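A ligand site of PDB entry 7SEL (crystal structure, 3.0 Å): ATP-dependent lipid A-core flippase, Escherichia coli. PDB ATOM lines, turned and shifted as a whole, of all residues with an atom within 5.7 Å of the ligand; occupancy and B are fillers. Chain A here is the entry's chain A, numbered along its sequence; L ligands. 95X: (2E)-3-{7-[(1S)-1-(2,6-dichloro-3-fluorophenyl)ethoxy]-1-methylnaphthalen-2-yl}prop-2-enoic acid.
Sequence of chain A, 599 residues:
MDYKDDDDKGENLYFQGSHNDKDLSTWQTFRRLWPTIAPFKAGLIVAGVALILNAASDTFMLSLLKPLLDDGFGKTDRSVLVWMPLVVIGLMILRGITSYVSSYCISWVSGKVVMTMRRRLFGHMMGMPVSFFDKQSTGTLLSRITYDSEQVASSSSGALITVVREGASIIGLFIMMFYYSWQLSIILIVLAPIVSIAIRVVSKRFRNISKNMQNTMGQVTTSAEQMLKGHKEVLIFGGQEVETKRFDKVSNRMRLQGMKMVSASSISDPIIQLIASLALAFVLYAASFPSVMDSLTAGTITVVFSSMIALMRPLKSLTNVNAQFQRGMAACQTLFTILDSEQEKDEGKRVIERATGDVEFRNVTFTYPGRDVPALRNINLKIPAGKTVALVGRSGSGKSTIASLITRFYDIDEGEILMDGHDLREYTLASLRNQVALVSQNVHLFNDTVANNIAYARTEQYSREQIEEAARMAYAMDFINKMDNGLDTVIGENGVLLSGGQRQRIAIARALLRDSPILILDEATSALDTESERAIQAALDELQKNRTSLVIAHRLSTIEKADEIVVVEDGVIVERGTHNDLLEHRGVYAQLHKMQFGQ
OG of Ser 196 sits at hydrogen-bond distance from O of Ala 192 (2.5 Å).
OG1 of Thr 319 is in hydrogen-bond range of O of Lys 316 (3.4 Å).
The backbone carbonyl oxygen (O) of Lys 316 lies close to the side-chain amide oxygen (OD1) of Asn 320, 2.8 Å away.
The backbone carbonyl oxygen (O) of Leu 315 lies within hydrogen-bond range of the side-chain hydroxyl (OG1) of Thr 319 (2.9 Å).
The guanidinium group (NH2) of Arg 207 is in salt-bridge range of an oxygen (O03) of the ligand, 3.3 Å away.
NZ of Lys 316 is in salt-bridge range of O03 of the ligand (3.3 Å).
A fluorine (F01) of the ligand sits close to the backbone carbonyl oxygen of Met 308.
Leu 188 touches the ligand (CD2 to C16, 3.4 Å).
Leu 191 touches the ligand (C to C13, 3.9 Å).
Ala 192 touches the ligand.
CG1 of Val 195 touches C12 of the ligand, at 3.8 Å.
OG of Ser 196 touches C10 of the ligand, at 2.9 Å.
Ile 199 touches the ligand.
Ile 272 touches the ligand.
Ala 276 touches the ligand (CB to CL01, 3.4 Å).
CD2 of Leu 280 touches F01 of the ligand (3.6 Å).
CD1 of Leu 311 touches C16 of the ligand (3.7 Å).
CG of Met 312 touches F01 of the ligand, 3.2 Å away.
CD1 of Leu 315 touches C16 of the ligand (3.6 Å).
Thr 319 touches the ligand (OG1 to C04, 3.8 Å).
Hydrophobic or aromatic side chains within 4 Å of the ligand: Leu 188, Ala 192, Val 195, Ile 199, Ile 272, Ala 276, Leu 280, Leu 311, Met 312 and Leu 315.
Of the 25 residues printed, 16 come within 4 Å of the ligand.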
ATOM      1  N   PHE A 174      12.716 -21.626   8.211  1.00  0.00           N
ATOM      2  CA  PHE A 174      13.008 -23.049   8.061  1.00  0.00           C
ATOM      3  C   PHE A 174      12.316 -23.622   6.827  1.00  0.00           C
ATOM      4  O   PHE A 174      12.939 -24.331   6.027  1.00  0.00           O
ATOM      5  CB  PHE A 174      12.568 -23.800   9.314  1.00  0.00           C
ATOM      6  CG  PHE A 174      13.668 -24.018  10.329  1.00  0.00           C
ATOM      7  CD1 PHE A 174      14.949 -24.366   9.929  1.00  0.00           C
ATOM      8  CD2 PHE A 174      13.413 -23.885  11.678  1.00  0.00           C
ATOM      9  CE1 PHE A 174      15.955 -24.559  10.862  1.00  0.00           C
ATOM     10  CE2 PHE A 174      14.412 -24.089  12.617  1.00  0.00           C
ATOM     11  CZ  PHE A 174      15.676 -24.425  12.204  1.00  0.00           C
ATOM     12  N   LEU A 188      22.527 -27.819   8.336  1.00  0.00           N
ATOM     13  CA  LEU A 188      22.345 -26.893   9.441  1.00  0.00           C
ATOM     14  C   LEU A 188      21.665 -27.585  10.616  1.00  0.00           C
ATOM     15  O   LEU A 188      22.067 -27.411  11.774  1.00  0.00           O
ATOM     16  CB  LEU A 188      21.517 -25.700   8.982  1.00  0.00           C
ATOM     17  CG  LEU A 188      21.712 -24.375   9.700  1.00  0.00           C
ATOM     18  CD1 LEU A 188      23.098 -23.827   9.454  1.00  0.00           C
ATOM     19  CD2 LEU A 188      20.664 -23.396   9.227  1.00  0.00           C
ATOM     20  N   ILE A 189      20.636 -28.380  10.334  1.00  0.00           N
ATOM     21  CA  ILE A 189      19.830 -28.978  11.399  1.00  0.00           C
ATOM     22  C   ILE A 189      20.659 -29.959  12.218  1.00  0.00           C
ATOM     23  O   ILE A 189      20.595 -29.959  13.455  1.00  0.00           O
ATOM     24  CB  ILE A 189      18.572 -29.637  10.814  1.00  0.00           C
ATOM     25  CG1 ILE A 189      17.441 -28.616  10.739  1.00  0.00           C
ATOM     26  CG2 ILE A 189      18.113 -30.836  11.646  1.00  0.00           C
ATOM     27  CD1 ILE A 189      17.707 -27.449   9.819  1.00  0.00           C
ATOM     28  N   LEU A 191      23.827 -29.948  12.629  1.00  0.00           N
ATOM     29  CA  LEU A 191      24.730 -29.143  13.425  1.00  0.00           C
ATOM     30  C   LEU A 191      24.031 -28.467  14.602  1.00  0.00           C
ATOM     31  O   LEU A 191      24.692 -28.052  15.546  1.00  0.00           O
ATOM     32  CB  LEU A 191      25.404 -28.087  12.548  1.00  0.00           C
ATOM     33  CG  LEU A 191      26.706 -28.487  11.851  1.00  0.00           C
ATOM     34  CD1 LEU A 191      27.096 -27.447  10.806  1.00  0.00           C
ATOM     35  CD2 LEU A 191      27.817 -28.644  12.867  1.00  0.00           C
ATOM     36  N   ALA A 192      22.698 -28.373  14.558  1.00  0.00           N
ATOM     37  CA  ALA A 192      21.982 -27.537  15.509  1.00  0.00           C
ATOM     38  C   ALA A 192      22.153 -27.973  16.957  1.00  0.00           C
ATOM     39  O   ALA A 192      22.371 -27.101  17.817  1.00  0.00           O
ATOM     40  CB  ALA A 192      20.501 -27.482  15.142  1.00  0.00           C
ATOM     41  N   PRO A 193      22.059 -29.257  17.316  1.00  0.00           N
ATOM     42  CA  PRO A 193      22.119 -29.588  18.747  1.00  0.00           C
ATOM     43  C   PRO A 193      23.473 -29.311  19.376  1.00  0.00           C
ATOM     44  O   PRO A 193      23.530 -28.789  20.494  1.00  0.00           O
ATOM     45  CB  PRO A 193      21.767 -31.089  18.770  1.00  0.00           C
ATOM     46  CG  PRO A 193      21.099 -31.345  17.462  1.00  0.00           C
ATOM     47  CD  PRO A 193      21.782 -30.440  16.489  1.00  0.00           C
ATOM     48  N   VAL A 195      25.794 -27.181  18.273  1.00  0.00           N
ATOM     49  CA  VAL A 195      25.958 -25.733  18.296  1.00  0.00           C
ATOM     50  C   VAL A 195      25.174 -25.148  19.457  1.00  0.00           C
ATOM     51  O   VAL A 195      25.653 -24.252  20.178  1.00  0.00           O
ATOM     52  CB  VAL A 195      25.522 -25.121  16.957  1.00  0.00           C
ATOM     53  CG1 VAL A 195      25.520 -23.589  17.009  1.00  0.00           C
ATOM     54  CG2 VAL A 195      26.438 -25.600  15.838  1.00  0.00           C
ATOM     55  N   SER A 196      23.947 -25.635  19.671  1.00  0.00           N
ATOM     56  CA  SER A 196      23.116 -25.140  20.762  1.00  0.00           C
ATOM     57  C   SER A 196      23.776 -25.405  22.106  1.00  0.00           C
ATOM     58  O   SER A 196      23.821 -24.522  22.964  1.00  0.00           O
ATOM     59  CB  SER A 196      21.750 -25.813  20.701  1.00  0.00           C
ATOM     60  OG  SER A 196      21.147 -25.597  19.438  1.00  0.00           O
ATOM     61  N   ILE A 199      26.750 -23.070  22.602  1.00  0.00           N
ATOM     62  CA  ILE A 199      26.343 -21.702  22.896  1.00  0.00           C
ATOM     63  C   ILE A 199      25.808 -21.606  24.316  1.00  0.00           C
ATOM     64  O   ILE A 199      26.108 -20.650  25.046  1.00  0.00           O
ATOM     65  CB  ILE A 199      25.300 -21.228  21.877  1.00  0.00           C
ATOM     66  CG1 ILE A 199      25.937 -21.145  20.481  1.00  0.00           C
ATOM     67  CG2 ILE A 199      24.740 -19.887  22.277  1.00  0.00           C
ATOM     68  CD1 ILE A 199      24.952 -20.937  19.355  1.00  0.00           C
ATOM     69  N   ARG A 207      27.956 -15.070  31.461  1.00  0.00           N
ATOM     70  CA  ARG A 207      26.953 -14.038  31.659  1.00  0.00           C
ATOM     71  C   ARG A 207      25.798 -14.570  32.507  1.00  0.00           C
ATOM     72  O   ARG A 207      24.860 -15.188  32.013  1.00  0.00           O
ATOM     73  CB  ARG A 207      26.466 -13.485  30.326  1.00  0.00           C
ATOM     74  CG  ARG A 207      25.959 -14.506  29.310  1.00  0.00           C
ATOM     75  CD  ARG A 207      25.955 -13.860  27.936  1.00  0.00           C
ATOM     76  NE  ARG A 207      25.342 -14.656  26.887  1.00  0.00           N
ATOM     77  CZ  ARG A 207      25.280 -14.284  25.607  1.00  0.00           C
ATOM     78  NH1 ARG A 207      25.792 -13.127  25.218  1.00  0.00           N
ATOM     79  NH2 ARG A 207      24.702 -15.074  24.707  1.00  0.00           N
ATOM     80  N   ASP A 269      29.789 -12.884  23.853  1.00  0.00           N
ATOM     81  CA  ASP A 269      29.118 -12.636  22.532  1.00  0.00           C
ATOM     82  C   ASP A 269      29.999 -13.038  21.382  1.00  0.00           C
ATOM     83  O   ASP A 269      29.557 -13.843  20.528  1.00  0.00           O
ATOM     84  CB  ASP A 269      28.705 -11.162  22.466  1.00  0.00           C
ATOM     85  CG  ASP A 269      27.667 -10.791  23.507  1.00  0.00           C
ATOM     86  OD1 ASP A 269      26.956 -11.700  23.987  1.00  0.00           O
ATOM     87  OD2 ASP A 269      27.560  -9.591  23.841  1.00  0.00           O
ATOM     88  N   ILE A 272      30.206 -16.729  20.907  1.00  0.00           N
ATOM     89  CA  ILE A 272      28.992 -17.406  20.482  1.00  0.00           C
ATOM     90  C   ILE A 272      28.779 -17.221  18.987  1.00  0.00           C
ATOM     91  O   ILE A 272      28.491 -18.184  18.258  1.00  0.00           O
ATOM     92  CB  ILE A 272      27.798 -16.904  21.310  1.00  0.00           C
ATOM     93  CG1 ILE A 272      27.870 -17.500  22.723  1.00  0.00           C
ATOM     94  CG2 ILE A 272      26.471 -17.266  20.649  1.00  0.00           C
ATOM     95  CD1 ILE A 272      26.827 -16.989  23.695  1.00  0.00           C
ATOM     96  N   ILE A 275      31.022 -19.535  17.144  1.00  0.00           N
ATOM     97  CA  ILE A 275      30.503 -20.912  17.052  1.00  0.00           C
ATOM     98  C   ILE A 275      29.512 -21.017  15.890  1.00  0.00           C
ATOM     99  O   ILE A 275      29.622 -21.900  15.018  1.00  0.00           O
ATOM    100  CB  ILE A 275      29.856 -21.317  18.395  1.00  0.00           C
ATOM    101  CG1 ILE A 275      30.884 -21.236  19.526  1.00  0.00           C
ATOM    102  CG2 ILE A 275      29.255 -22.719  18.333  1.00  0.00           C
ATOM    103  CD1 ILE A 275      30.301 -21.424  20.928  1.00  0.00           C
ATOM    104  N   ALA A 276      28.519 -20.117  15.878  1.00  0.00           N
ATOM    105  CA  ALA A 276      27.560 -20.116  14.780  1.00  0.00           C
ATOM    106  C   ALA A 276      28.262 -19.942  13.439  1.00  0.00           C
ATOM    107  O   ALA A 276      27.865 -20.559  12.434  1.00  0.00           O
ATOM    108  CB  ALA A 276      26.535 -19.006  14.990  1.00  0.00           C
ATOM    109  N   SER A 277      29.315 -19.126  13.408  1.00  0.00           N
ATOM    110  CA  SER A 277      30.076 -18.908  12.179  1.00  0.00           C
ATOM    111  C   SER A 277      30.694 -20.203  11.686  1.00  0.00           C
ATOM    112  O   SER A 277      30.719 -20.465  10.476  1.00  0.00           O
ATOM    113  CB  SER A 277      31.159 -17.867  12.439  1.00  0.00           C
ATOM    114  OG  SER A 277      31.789 -17.490  11.228  1.00  0.00           O
ATOM    115  N   ALA A 279      29.520 -23.273  12.192  1.00  0.00           N
ATOM    116  CA  ALA A 279      28.446 -24.081  11.596  1.00  0.00           C
ATOM    117  C   ALA A 279      28.130 -23.613  10.176  1.00  0.00           C
ATOM    118  O   ALA A 279      28.015 -24.426   9.241  1.00  0.00           O
ATOM    119  CB  ALA A 279      27.200 -24.017  12.473  1.00  0.00           C
ATOM    120  N   LEU A 280      28.004 -22.293   9.986  1.00  0.00           N
ATOM    121  CA  LEU A 280      27.666 -21.779   8.662  1.00  0.00           C
ATOM    122  C   LEU A 280      28.788 -22.029   7.656  1.00  0.00           C
ATOM    123  O   LEU A 280      28.521 -22.311   6.488  1.00  0.00           O
ATOM    124  CB  LEU A 280      27.353 -20.283   8.758  1.00  0.00           C
ATOM    125  CG  LEU A 280      26.071 -19.901   9.505  1.00  0.00           C
ATOM    126  CD1 LEU A 280      25.896 -18.396   9.439  1.00  0.00           C
ATOM    127  CD2 LEU A 280      24.858 -20.607   8.935  1.00  0.00           C
ATOM    128  N   MET A 308      19.384 -18.304   6.659  1.00  0.00           N
ATOM    129  CA  MET A 308      20.132 -18.821   7.801  1.00  0.00           C
ATOM    130  C   MET A 308      20.658 -17.684   8.675  1.00  0.00           C
ATOM    131  O   MET A 308      20.582 -17.750   9.901  1.00  0.00           O
ATOM    132  CB  MET A 308      21.271 -19.720   7.334  1.00  0.00           C
ATOM    133  CG  MET A 308      20.801 -20.944   6.582  1.00  0.00           C
ATOM    134  SD  MET A 308      22.171 -21.927   5.957  1.00  0.00           S
ATOM    135  CE  MET A 308      21.292 -23.362   5.369  1.00  0.00           C
ATOM    136  N   ILE A 309      21.211 -16.639   8.048  1.00  0.00           N
ATOM    137  CA  ILE A 309      21.675 -15.480   8.810  1.00  0.00           C
ATOM    138  C   ILE A 309      20.515 -14.879   9.603  1.00  0.00           C
ATOM    139  O   ILE A 309      20.616 -14.668  10.810  1.00  0.00           O
ATOM    140  CB  ILE A 309      22.311 -14.440   7.870  1.00  0.00           C
ATOM    141  CG1 ILE A 309      23.681 -14.923   7.405  1.00  0.00           C
ATOM    142  CG2 ILE A 309      22.444 -13.069   8.555  1.00  0.00           C
ATOM    143  CD1 ILE A 309      24.334 -14.054   6.318  1.00  0.00           C
ATOM    144  N   LEU A 311      18.000 -16.155  10.697  1.00  0.00           N
ATOM    145  CA  LEU A 311      17.569 -17.022  11.778  1.00  0.00           C
ATOM    146  C   LEU A 311      18.323 -16.774  13.082  1.00  0.00           C
ATOM    147  O   LEU A 311      17.797 -17.098  14.152  1.00  0.00           O
ATOM    148  CB  LEU A 311      17.745 -18.489  11.403  1.00  0.00           C
ATOM    149  CG  LEU A 311      16.586 -19.240  10.740  1.00  0.00           C
ATOM    150  CD1 LEU A 311      16.973 -20.700  10.565  1.00  0.00           C
ATOM    151  CD2 LEU A 311      15.311 -19.150  11.542  1.00  0.00           C
ATOM    152  N   MET A 312      19.522 -16.205  13.028  1.00  0.00           N
ATOM    153  CA  MET A 312      20.333 -16.096  14.229  1.00  0.00           C
ATOM    154  C   MET A 312      19.682 -15.195  15.259  1.00  0.00           C
ATOM    155  O   MET A 312      19.765 -15.455  16.467  1.00  0.00           O
ATOM    156  CB  MET A 312      21.738 -15.598  13.879  1.00  0.00           C
ATOM    157  CG  MET A 312      22.574 -16.628  13.124  1.00  0.00           C
ATOM    158  SD  MET A 312      24.292 -16.129  12.885  1.00  0.00           S
ATOM    159  CE  MET A 312      24.098 -14.680  11.858  1.00  0.00           C
ATOM    160  N   LEU A 315      16.654 -17.019  16.995  1.00  0.00           N
ATOM    161  CA  LEU A 315      17.106 -18.077  17.893  1.00  0.00           C
ATOM    162  C   LEU A 315      17.642 -17.470  19.191  1.00  0.00           C
ATOM    163  O   LEU A 315      17.339 -17.958  20.293  1.00  0.00           O
ATOM    164  CB  LEU A 315      18.182 -18.911  17.202  1.00  0.00           C
ATOM    165  CG  LEU A 315      17.714 -19.705  15.971  1.00  0.00           C
ATOM    166  CD1 LEU A 315      18.889 -20.343  15.239  1.00  0.00           C
ATOM    167  CD2 LEU A 315      16.704 -20.774  16.359  1.00  0.00           C
ATOM    168  N   LYS A 316      18.456 -16.427  19.077  1.00  0.00           N
ATOM    169  CA  LYS A 316      18.917 -15.694  20.249  1.00  0.00           C
ATOM    170  C   LYS A 316      17.729 -15.223  21.079  1.00  0.00           C
ATOM    171  O   LYS A 316      17.672 -15.471  22.290  1.00  0.00           O
ATOM    172  CB  LYS A 316      19.773 -14.500  19.821  1.00  0.00           C
ATOM    173  CG  LYS A 316      20.075 -13.510  20.945  1.00  0.00           C
ATOM    174  CD  LYS A 316      21.115 -12.476  20.533  1.00  0.00           C
ATOM    175  CE  LYS A 316      21.479 -11.545  21.685  1.00  0.00           C
ATOM    176  NZ  LYS A 316      22.041 -12.285  22.843  1.00  0.00           N
ATOM    177  N   THR A 319      15.803 -18.279  22.844  1.00  0.00           N
ATOM    178  CA  THR A 319      16.414 -19.009  23.963  1.00  0.00           C
ATOM    179  C   THR A 319      16.655 -18.124  25.234  1.00  0.00           C
ATOM    180  O   THR A 319      17.344 -18.615  26.136  1.00  0.00           O
ATOM    181  CB  THR A 319      17.732 -19.679  23.524  1.00  0.00           C
ATOM    182  OG1 THR A 319      18.536 -18.733  22.821  1.00  0.00           O
ATOM    183  CG2 THR A 319      17.452 -20.887  22.641  1.00  0.00           C
ATOM    184  N   ASN A 320      16.139 -16.895  25.338  1.00  0.00           N
ATOM    185  CA  ASN A 320      16.223 -16.074  26.550  1.00  0.00           C
ATOM    186  C   ASN A 320      14.840 -15.716  27.104  1.00  0.00           C
ATOM    187  O   ASN A 320      14.718 -14.940  28.078  1.00  0.00           O
ATOM    188  CB  ASN A 320      17.033 -14.817  26.249  1.00  0.00           C
ATOM    189  CG  ASN A 320      18.425 -15.140  25.744  1.00  0.00           C
ATOM    190  OD1 ASN A 320      18.827 -14.690  24.663  1.00  0.00           O
ATOM    191  ND2 ASN A 320      19.167 -15.936  26.502  1.00  0.00           N
HETATM  192  C12 95X L   1      22.730 -23.493  14.473  1.00  0.00           C
HETATM  193  C11 95X L   1      20.451 -22.597  18.646  1.00  0.00           C
HETATM  194  C10 95X L   1      20.800 -23.430  17.582  1.00  0.00           C
HETATM  195  C01 95X L   1      23.062 -18.814  16.681  1.00  0.00           C
HETATM  196  C02 95X L   1      22.176 -19.378  17.781  1.00  0.00           C
HETATM  197  C03 95X L   1      21.775 -18.589  18.891  1.00  0.00           C
HETATM  198  C04 95X L   1      20.967 -19.143  19.876  1.00  0.00           C
HETATM  199  C05 95X L   1      20.536 -20.465  19.793  1.00  0.00           C
HETATM  200  C06 95X L   1      20.908 -21.274  18.712  1.00  0.00           C
HETATM  201  C07 95X L   1      21.737 -20.746  17.677  1.00  0.00           C
HETATM  202  C08 95X L   1      22.071 -21.618  16.613  1.00  0.00           C
HETATM  203  C09 95X L   1      21.620 -22.945  16.560  1.00  0.00           C
HETATM  204  C13 95X L   1      23.153 -24.768  13.751  1.00  0.00           C
HETATM  205  C14 95X L   1      22.049 -22.543  13.498  1.00  0.00           C
HETATM  206  C15 95X L   1      20.720 -22.727  13.068  1.00  0.00           C
HETATM  207  C16 95X L   1      20.099 -21.847  12.172  1.00  0.00           C
HETATM  208  C17 95X L   1      20.794 -20.741  11.688  1.00  0.00           C
HETATM  209  C18 95X L   1      22.101 -20.541  12.092  1.00  0.00           C
HETATM  210  C19 95X L   1      22.733 -21.414  12.993  1.00  0.00           C
HETATM  211  C20 95X L   1      22.198 -17.182  19.070  1.00  0.00           C
HETATM  212  C21 95X L   1      22.767 -16.776  20.222  1.00  0.00           C
HETATM  213  C22 95X L   1      23.244 -15.358  20.440  1.00  0.00           C
HETATM  214  F01 95X L   1      22.762 -19.476  11.613  1.00  0.00           F
HETATM  215  O01 95X L   1      21.883 -23.860  15.579  1.00  0.00           O
HETATM  216  O02 95X L   1      23.388 -14.641  19.408  1.00  0.00           O
HETATM  217  O03 95X L   1      23.461 -15.032  21.643  1.00  0.00           O
HETATM  218 CL01 95X L   1      24.369 -21.027  13.400  1.00  0.00          CL
HETATM  219 CL02 95X L   1      19.677 -24.028  13.546  1.00  0.00          CL
